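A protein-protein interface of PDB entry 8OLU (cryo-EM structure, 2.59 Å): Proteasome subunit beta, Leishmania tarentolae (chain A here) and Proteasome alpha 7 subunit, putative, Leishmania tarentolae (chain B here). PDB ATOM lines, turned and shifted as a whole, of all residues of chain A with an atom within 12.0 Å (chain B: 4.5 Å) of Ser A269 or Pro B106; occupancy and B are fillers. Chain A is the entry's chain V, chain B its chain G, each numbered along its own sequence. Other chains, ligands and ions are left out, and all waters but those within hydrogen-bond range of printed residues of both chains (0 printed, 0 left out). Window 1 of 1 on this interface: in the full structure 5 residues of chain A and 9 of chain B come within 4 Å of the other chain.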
ATOM      1  N   THR A 263      -0.196  15.554 -26.968  1.00  0.00           N
ATOM      2  CA  THR A 263      -0.332  14.382 -26.120  1.00  0.00           C
ATOM      3  C   THR A 263       1.014  14.067 -25.479  1.00  0.00           C
ATOM      4  O   THR A 263       1.845  13.378 -26.069  1.00  0.00           O
ATOM      5  CB  THR A 263      -0.775  13.195 -26.956  1.00  0.00           C
ATOM      6  OG1 THR A 263      -2.062  13.401 -27.522  1.00  0.00           O
ATOM      7  CG2 THR A 263      -0.827  12.009 -26.046  1.00  0.00           C
ATOM      8  N   GLN A 264       1.260  14.687 -24.334  1.00  0.00           N
ATOM      9  CA  GLN A 264       2.566  14.678 -23.712  1.00  0.00           C
ATOM     10  C   GLN A 264       2.546  13.905 -22.430  1.00  0.00           C
ATOM     11  O   GLN A 264       3.585  13.627 -21.882  1.00  0.00           O
ATOM     12  CB  GLN A 264       2.987  16.058 -23.225  1.00  0.00           C
ATOM     13  CG  GLN A 264       3.224  17.017 -24.340  1.00  0.00           C
ATOM     14  CD  GLN A 264       4.430  16.653 -25.167  1.00  0.00           C
ATOM     15  OE1 GLN A 264       4.265  16.077 -26.231  1.00  0.00           O
ATOM     16  NE2 GLN A 264       5.618  17.003 -24.699  1.00  0.00           N
ATOM     17  N   ASN A 265       1.390  13.813 -21.830  1.00  0.00           N
ATOM     18  CA  ASN A 265       1.315  13.318 -20.491  1.00  0.00           C
ATOM     19  C   ASN A 265       0.472  12.062 -20.557  1.00  0.00           C
ATOM     20  O   ASN A 265      -0.634  12.023 -20.017  1.00  0.00           O
ATOM     21  CB  ASN A 265       0.599  14.311 -19.598  1.00  0.00           C
ATOM     22  CG  ASN A 265       1.315  15.626 -19.460  1.00  0.00           C
ATOM     23  OD1 ASN A 265       2.546  15.669 -19.488  1.00  0.00           O
ATOM     24  ND2 ASN A 265       0.527  16.667 -19.232  1.00  0.00           N
ATOM     25  N   GLN A 266       0.977  11.085 -21.291  1.00  0.00           N
ATOM     26  CA  GLN A 266       0.243   9.871 -21.517  1.00  0.00           C
ATOM     27  C   GLN A 266       0.079   9.169 -20.199  1.00  0.00           C
ATOM     28  O   GLN A 266       0.962   9.214 -19.372  1.00  0.00           O
ATOM     29  CB  GLN A 266       1.037   8.962 -22.428  1.00  0.00           C
ATOM     30  CG  GLN A 266       0.947   9.289 -23.909  1.00  0.00           C
ATOM     31  CD  GLN A 266       1.954   8.389 -24.589  1.00  0.00           C
ATOM     32  OE1 GLN A 266       1.933   7.163 -24.420  1.00  0.00           O
ATOM     33  NE2 GLN A 266       2.905   8.992 -25.276  1.00  0.00           N
ATOM     34  N   PRO A 267      -1.021   8.470 -19.959  1.00  0.00           N
ATOM     35  CA  PRO A 267      -1.098   7.590 -18.809  1.00  0.00           C
ATOM     36  C   PRO A 267      -0.263   6.365 -19.052  1.00  0.00           C
ATOM     37  O   PRO A 267      -0.205   5.881 -20.188  1.00  0.00           O
ATOM     38  CB  PRO A 267      -2.497   7.004 -18.755  1.00  0.00           C
ATOM     39  CG  PRO A 267      -3.131   7.423 -20.040  1.00  0.00           C
ATOM     40  CD  PRO A 267      -2.211   8.413 -20.777  1.00  0.00           C
ATOM     41  N   PHE A 268       0.222   5.828 -17.930  1.00  0.00           N
ATOM     42  CA  PHE A 268       0.926   4.556 -17.837  1.00  0.00           C
ATOM     43  C   PHE A 268       0.075   3.446 -18.416  1.00  0.00           C
ATOM     44  O   PHE A 268      -1.056   3.243 -17.968  1.00  0.00           O
ATOM     45  CB  PHE A 268       1.131   4.237 -16.367  1.00  0.00           C
ATOM     46  CG  PHE A 268       2.192   3.222 -16.097  1.00  0.00           C
ATOM     47  CD1 PHE A 268       3.427   3.316 -16.709  1.00  0.00           C
ATOM     48  CD2 PHE A 268       1.968   2.223 -15.172  1.00  0.00           C
ATOM     49  CE1 PHE A 268       4.403   2.367 -16.459  1.00  0.00           C
ATOM     50  CE2 PHE A 268       2.956   1.305 -14.912  1.00  0.00           C
ATOM     51  CZ  PHE A 268       4.162   1.364 -15.573  1.00  0.00           C
ATOM     52  N   SER A 269       0.568   2.809 -19.484  1.00  0.00           N
ATOM     53  CA  SER A 269      -0.257   1.791 -20.090  1.00  0.00           C
ATOM     54  C   SER A 269       0.548   0.551 -20.442  1.00  0.00           C
ATOM     55  O   SER A 269       1.767   0.568 -20.500  1.00  0.00           O
ATOM     56  CB  SER A 269      -1.027   2.358 -21.250  1.00  0.00           C
ATOM     57  OG  SER A 269      -0.361   2.176 -22.475  1.00  0.00           O
ATOM     58  N   SER A 270      -0.205  -0.502 -20.729  1.00  0.00           N
ATOM     59  CA  SER A 270       0.340  -1.758 -21.168  1.00  0.00           C
ATOM     60  C   SER A 270       0.548  -1.729 -22.680  1.00  0.00           C
ATOM     61  O   SER A 270       1.005  -2.698 -23.281  1.00  0.00           O
ATOM     62  CB  SER A 270      -0.607  -2.824 -20.762  1.00  0.00           C
ATOM     63  OG  SER A 270      -0.906  -2.723 -19.359  1.00  0.00           O
ATOM     64  N   SER A 271       0.199  -0.623 -23.329  1.00  0.00           N
ATOM     65  CA  SER A 271       0.355  -0.577 -24.764  1.00  0.00           C
ATOM     66  C   SER A 271       1.145   0.658 -25.186  1.00  0.00           C
ATOM     67  O   SER A 271       1.366   1.588 -24.418  1.00  0.00           O
ATOM     68  CB  SER A 271      -0.977  -0.663 -25.460  1.00  0.00           C
ATOM     69  OG  SER A 271      -0.857  -0.475 -26.865  1.00  0.00           O
ATOM     70  N   ALA A 272       1.646   0.588 -26.418  1.00  0.00           N
ATOM     71  CA  ALA A 272       2.244   1.719 -27.080  1.00  0.00           C
ATOM     72  C   ALA A 272       1.198   2.627 -27.740  1.00  0.00           C
ATOM     73  O   ALA A 272       1.546   3.735 -28.174  1.00  0.00           O
ATOM     74  CB  ALA A 272       3.210   1.206 -28.098  1.00  0.00           C
ATOM     75  N   LYS A 273      -0.036   2.124 -27.891  1.00  0.00           N
ATOM     76  CA  LYS A 273      -1.111   2.909 -28.469  1.00  0.00           C
ATOM     77  C   LYS A 273      -1.331   4.135 -27.590  1.00  0.00           C
ATOM     78  O   LYS A 273      -1.583   4.019 -26.392  1.00  0.00           O
ATOM     79  CB  LYS A 273      -2.357   2.039 -28.612  1.00  0.00           C
ATOM     80  CG  LYS A 273      -3.642   2.740 -29.011  1.00  0.00           C
ATOM     81  CD  LYS A 273      -3.480   3.667 -30.193  1.00  0.00           C
ATOM     82  CE  LYS A 273      -4.778   4.326 -30.619  1.00  0.00           C
ATOM     83  NZ  LYS A 273      -5.613   3.337 -31.341  1.00  0.00           N
ATOM     84  N   ILE A 274      -1.163   5.291 -28.212  1.00  0.00           N
ATOM     85  CA  ILE A 274      -1.360   6.598 -27.635  1.00  0.00           C
ATOM     86  C   ILE A 274      -2.843   6.979 -27.647  1.00  0.00           C
ATOM     87  O   ILE A 274      -3.534   6.878 -28.659  1.00  0.00           O
ATOM     88  CB  ILE A 274      -0.490   7.582 -28.429  1.00  0.00           C
ATOM     89  CG1 ILE A 274       0.969   7.459 -28.000  1.00  0.00           C
ATOM     90  CG2 ILE A 274      -0.972   8.991 -28.288  1.00  0.00           C
ATOM     91  CD1 ILE A 274       1.951   8.122 -28.927  1.00  0.00           C
ATOM     92  N   THR A 275      -3.309   7.456 -26.489  1.00  0.00           N
ATOM     93  CA  THR A 275      -4.730   7.662 -26.239  1.00  0.00           C
ATOM     94  C   THR A 275      -5.002   9.161 -26.123  1.00  0.00           C
ATOM     95  O   THR A 275      -5.954   9.675 -26.707  1.00  0.00           O
ATOM     96  CB  THR A 275      -5.219   6.833 -25.021  1.00  0.00           C
ATOM     97  OG1 THR A 275      -4.470   7.068 -23.819  1.00  0.00           O
ATOM     98  CG2 THR A 275      -5.153   5.339 -25.304  1.00  0.00           C
ATOM     99  N   GLY A 276      -4.150   9.880 -25.397  1.00  0.00           N
ATOM    100  CA  GLY A 276      -4.623  11.086 -24.758  1.00  0.00           C
ATOM    101  C   GLY A 276      -3.779  11.451 -23.552  1.00  0.00           C
ATOM    102  O   GLY A 276      -2.850  10.762 -23.189  1.00  0.00           O
ATOM    103  N   ASN A 277      -4.034  12.623 -23.014  1.00  0.00           N
ATOM    104  CA  ASN A 277      -3.306  13.033 -21.853  1.00  0.00           C
ATOM    105  C   ASN A 277      -4.055  12.481 -20.665  1.00  0.00           C
ATOM    106  O   ASN A 277      -5.259  12.327 -20.731  1.00  0.00           O
ATOM    107  CB  ASN A 277      -3.199  14.540 -21.815  1.00  0.00           C
ATOM    108  CG  ASN A 277      -2.239  15.062 -22.837  1.00  0.00           C
ATOM    109  OD1 ASN A 277      -1.074  14.699 -22.781  1.00  0.00           O
ATOM    110  ND2 ASN A 277      -2.692  15.942 -23.710  1.00  0.00           N
ATOM    111  N   ARG A 278      -3.324  12.218 -19.595  1.00  0.00           N
ATOM    112  CA  ARG A 278      -3.954  11.781 -18.380  1.00  0.00           C
ATOM    113  C   ARG A 278      -4.529  13.009 -17.691  1.00  0.00           C
ATOM    114  O   ARG A 278      -3.791  13.825 -17.177  1.00  0.00           O
ATOM    115  CB  ARG A 278      -2.918  11.002 -17.565  1.00  0.00           C
ATOM    116  CG  ARG A 278      -3.402  10.534 -16.201  1.00  0.00           C
ATOM    117  CD  ARG A 278      -2.241   9.932 -15.443  1.00  0.00           C
ATOM    118  NE  ARG A 278      -2.830   9.359 -14.234  1.00  0.00           N
ATOM    119  CZ  ARG A 278      -2.296   9.425 -13.025  1.00  0.00           C
ATOM    120  NH1 ARG A 278      -3.008   9.090 -11.963  1.00  0.00           N
ATOM    121  NH2 ARG A 278      -1.045   9.829 -12.906  1.00  0.00           N
ATOM    122  N   SER A 280      -6.901  12.967 -15.123  1.00  0.00           N
ATOM    123  CA  SER A 280      -7.459  12.746 -13.809  1.00  0.00           C
ATOM    124  C   SER A 280      -6.688  11.623 -13.168  1.00  0.00           C
ATOM    125  O   SER A 280      -6.097  10.851 -13.881  1.00  0.00           O
ATOM    126  CB  SER A 280      -8.913  12.484 -13.947  1.00  0.00           C
ATOM    127  OG  SER A 280      -9.332  11.390 -13.148  1.00  0.00           O
ATOM    128  N   SER A 281      -6.657  11.570 -11.839  1.00  0.00           N
ATOM    129  CA  SER A 281      -5.804  10.650 -11.105  1.00  0.00           C
ATOM    130  C   SER A 281      -6.335   9.242 -11.200  1.00  0.00           C
ATOM    131  O   SER A 281      -5.572   8.337 -11.534  1.00  0.00           O
ATOM    132  CB  SER A 281      -5.617  11.055  -9.703  1.00  0.00           C
ATOM    133  OG  SER A 281      -4.558  12.024  -9.623  1.00  0.00           O
ATOM    134  N   THR A 282      -7.642   9.102 -10.933  1.00  0.00           N
ATOM    135  CA  THR A 282      -8.386   7.845 -11.058  1.00  0.00           C
ATOM    136  C   THR A 282      -8.086   7.147 -12.406  1.00  0.00           C
ATOM    137  O   THR A 282      -8.287   7.793 -13.472  1.00  0.00           O
ATOM    138  CB  THR A 282      -9.897   8.108 -10.884  1.00  0.00           C
ATOM    139  OG1 THR A 282     -10.393   8.682 -12.095  1.00  0.00           O
ATOM    140  CG2 THR A 282     -10.246   9.019  -9.715  1.00  0.00           C
ATOM    141  N   ASP B  71       6.158  -5.387 -14.703  1.00  0.00           N
ATOM    142  CA  ASP B  71       5.808  -4.157 -15.352  1.00  0.00           C
ATOM    143  C   ASP B  71       4.309  -4.068 -15.238  1.00  0.00           C
ATOM    144  O   ASP B  71       3.703  -4.989 -14.721  1.00  0.00           O
ATOM    145  CB  ASP B  71       6.209  -4.154 -16.814  1.00  0.00           C
ATOM    146  CG  ASP B  71       6.270  -2.749 -17.453  1.00  0.00           C
ATOM    147  OD1 ASP B  71       6.057  -1.682 -16.702  1.00  0.00           O
ATOM    148  OD2 ASP B  71       6.664  -2.673 -18.737  1.00  0.00           O
ATOM    149  N   ARG B  72       3.697  -3.024 -15.777  1.00  0.00           N
ATOM    150  CA  ARG B  72       2.255  -2.957 -15.714  1.00  0.00           C
ATOM    151  C   ARG B  72       1.665  -4.201 -16.350  1.00  0.00           C
ATOM    152  O   ARG B  72       0.779  -4.797 -15.806  1.00  0.00           O
ATOM    153  CB  ARG B  72       1.762  -1.676 -16.375  1.00  0.00           C
ATOM    154  CG  ARG B  72       0.266  -1.419 -16.200  1.00  0.00           C
ATOM    155  CD  ARG B  72      -0.249  -0.193 -16.944  1.00  0.00           C
ATOM    156  NE  ARG B  72      -1.598   0.177 -16.539  1.00  0.00           N
ATOM    157  CZ  ARG B  72      -2.683  -0.495 -16.922  1.00  0.00           C
ATOM    158  NH1 ARG B  72      -3.798  -0.479 -16.202  1.00  0.00           N
ATOM    159  NH2 ARG B  72      -2.582  -1.339 -17.933  1.00  0.00           N
ATOM    160  N   GLN B  73       2.216  -4.647 -17.455  1.00  0.00           N
ATOM    161  CA  GLN B  73       1.521  -5.622 -18.247  1.00  0.00           C
ATOM    162  C   GLN B  73       2.113  -7.009 -18.141  1.00  0.00           C
ATOM    163  O   GLN B  73       1.822  -7.861 -18.949  1.00  0.00           O
ATOM    164  CB  GLN B  73       1.622  -5.166 -19.684  1.00  0.00           C
ATOM    165  CG  GLN B  73       2.971  -5.294 -20.359  1.00  0.00           C
ATOM    166  CD  GLN B  73       3.965  -4.258 -19.896  1.00  0.00           C
ATOM    167  OE1 GLN B  73       3.588  -3.222 -19.324  1.00  0.00           O
ATOM    168  NE2 GLN B  73       5.256  -4.534 -20.131  1.00  0.00           N
ATOM    169  N   SER B  99      12.998  -0.742 -21.309  1.00  0.00           N
ATOM    170  CA  SER B  99      12.197  -0.624 -22.499  1.00  0.00           C
ATOM    171  C   SER B  99      11.405   0.666 -22.385  1.00  0.00           C
ATOM    172  O   SER B  99      11.305   1.407 -23.335  1.00  0.00           O
ATOM    173  CB  SER B  99      11.323  -1.838 -22.732  1.00  0.00           C
ATOM    174  OG  SER B  99      10.452  -1.592 -23.846  1.00  0.00           O
ATOM    175  N   ARG B 100      10.876   0.998 -21.224  1.00  0.00           N
ATOM    176  CA  ARG B 100      10.087   2.211 -21.116  1.00  0.00           C
ATOM    177  C   ARG B 100      10.924   3.483 -21.128  1.00  0.00           C
ATOM    178  O   ARG B 100      10.475   4.515 -21.621  1.00  0.00           O
ATOM    179  CB  ARG B 100       9.249   2.181 -19.868  1.00  0.00           C
ATOM    180  CG  ARG B 100       7.998   1.398 -20.169  1.00  0.00           C
ATOM    181  CD  ARG B 100       7.283   1.214 -18.855  1.00  0.00           C
ATOM    182  NE  ARG B 100       6.201   0.272 -19.028  1.00  0.00           N
ATOM    183  CZ  ARG B 100       5.027   0.560 -19.545  1.00  0.00           C
ATOM    184  NH1 ARG B 100       4.744   1.779 -19.998  1.00  0.00           N
ATOM    185  NH2 ARG B 100       4.134  -0.404 -19.524  1.00  0.00           N
ATOM    186  N   THR B 105       8.238   2.360 -24.795  1.00  0.00           N
ATOM    187  CA  THR B 105       7.257   1.374 -25.170  1.00  0.00           C
ATOM    188  C   THR B 105       7.311   0.370 -24.039  1.00  0.00           C
ATOM    189  O   THR B 105       8.404   0.092 -23.533  1.00  0.00           O
ATOM    190  CB  THR B 105       7.558   0.757 -26.571  1.00  0.00           C
ATOM    191  OG1 THR B 105       6.519  -0.037 -27.178  1.00  0.00           O
ATOM    192  CG2 THR B 105       8.778  -0.159 -26.591  1.00  0.00           C
ATOM    193  N   PRO B 106       6.187  -0.259 -23.694  1.00  0.00           N
ATOM    194  CA  PRO B 106       6.223  -1.440 -22.873  1.00  0.00           C
ATOM    195  C   PRO B 106       6.923  -2.564 -23.580  1.00  0.00           C
ATOM    196  O   PRO B 106       6.722  -2.749 -24.753  1.00  0.00           O
ATOM    197  CB  PRO B 106       4.783  -1.887 -22.762  1.00  0.00           C
ATOM    198  CG  PRO B 106       4.035  -0.619 -23.123  1.00  0.00           C
ATOM    199  CD  PRO B 106       4.858  -0.010 -24.238  1.00  0.00           C
ATOM    200  N   ILE B 107       7.688  -3.329 -22.819  1.00  0.00           N
ATOM    201  CA  ILE B 107       8.461  -4.412 -23.360  1.00  0.00           C
ATOM    202  C   ILE B 107       7.481  -5.446 -23.844  1.00  0.00           C
ATOM    203  O   ILE B 107       6.603  -5.825 -23.100  1.00  0.00           O
ATOM    204  CB  ILE B 107       9.446  -4.978 -22.313  1.00  0.00           C
ATOM    205  CG1 ILE B 107      10.481  -5.893 -22.957  1.00  0.00           C
ATOM    206  CG2 ILE B 107       8.747  -5.731 -21.200  1.00  0.00           C
ATOM    207  CD1 ILE B 107      11.730  -6.099 -22.166  1.00  0.00           C
ATOM    208  N   ARG B 108       7.663  -5.888 -25.078  1.00  0.00           N
ATOM    209  CA  ARG B 108       6.895  -6.995 -25.576  1.00  0.00           C
ATOM    210  C   ARG B 108       7.241  -8.223 -24.746  1.00  0.00           C
ATOM    211  O   ARG B 108       8.326  -8.329 -24.231  1.00  0.00           O
ATOM    212  CB  ARG B 108       7.195  -7.231 -27.059  1.00  0.00           C
ATOM    213  CG  ARG B 108       6.707  -6.118 -27.983  1.00  0.00           C
ATOM    214  CD  ARG B 108       7.454  -6.163 -29.306  1.00  0.00           C
ATOM    215  NE  ARG B 108       6.867  -7.181 -30.155  1.00  0.00           N
ATOM    216  CZ  ARG B 108       5.793  -6.956 -30.896  1.00  0.00           C
ATOM    217  NH1 ARG B 108       5.058  -7.977 -31.310  1.00  0.00           N
ATOM    218  NH2 ARG B 108       5.450  -5.702 -31.153  1.00  0.00           N
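NE of Arg B72 is in hydrogen-bond range of O of Phe A268, 3.4 Å away. The guanidinium group (NH2) of Arg B72 is in hydrogen-bond range of the side-chain hydroxyl (OG) of Ser A270, at 2.6 Å. O of Ser A269 lies within hydrogen-bond range of NH2 of Arg B100, 2.7 Å away.
The side-chain carboxylate (OD2) of Asp B71 is in hydrogen-bond range of the side-chain amide nitrogen (NE2) of Gln B73 (2.7 Å). NE of Arg B100 lies within salt-bridge range of OD2 of Asp B71, 3.0 Å away. NH2 of Arg B100 sits at hydrogen-bond distance from OE1 of Gln B73, 2.9 Å away. The backbone carbonyl oxygen (O) of Thr B105 sits at hydrogen-bond distance from the side-chain hydroxyl (OG) of Ser B99, 2.7 Å away. The backbone carbonyl oxygen (O) of Ser A271 is in hydrogen-bond range of the side-chain hydroxyl (OG) of Ser A269 (2.7 Å). The side-chain hydroxyl (OG) of Ser A271 sits at hydrogen-bond distance from the backbone NH (N) of Lys A273 (2.9 Å).
Asp B71 touches Phe A268. NH1 of Arg B100 touches CE1 of Phe A268 (3.6 Å). Ser A269 touches Arg B72. O of Ser A269 touches CG of Pro B106, 3.7 Å away. Ser A270 touches Gln B73 (CB to CB, 3.4 Å). CG of Pro B106 touches O of Ser A270, 3.7 Å away. CG of Pro B106 touches O of Ser A271, at 3.7 Å. OG1 of Thr B105 touches CB of Ala A272, at 3.7 Å. N of Ala A272 touches CD of Pro B106, 3.9 Å away.
Of chain B, only Arg B72 (3.7 Å), Arg B100 (2.7 Å) and Pro B106 (3.7 Å) come within 4 Å of Ser A269. Printed residues of chain A within 4 Å of Pro B106: Ser A269, Ser A270, Ser A271 and Ala A272. Of chain A, only Phe A268, Ser A269 and Ser A270 come within 4 Å of Arg B72. Gln B73 touches just one residue of chain A: Ser A270. No residue of chain A comes within 4 Å of Ser B99. Arg B100 touches two residues of chain A. Thr B105 touches just one residue of chain A: Ala A272 (3.7 Å). No residue of chain A comes within 4 Å of Ile B107. Of the printed residues of chain B, Ser A271 touches Pro B106 (3.7 Å). Of the printed residues of chain A, Asp B71 touches Phe A268. Of the printed residues of chain B, Ala A272 touches Thr B105 (3.7 Å) and Pro B106 (3.9 Å).
Hydrophobic or aromatic side chains of chain B that line the printed part of chain A: Pro B106. Printed residues of chain A that touch a printed residue of chain B: Phe A268, Ser A269, Ser A270, Ser A271 and Ala A272. Among the printed residues, 12 pairs touch across the chains. Among the printed residues, no Asp or Glu carboxylate lies within 4 Å of a Lys or Arg side-chain nitrogen of the other chain.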
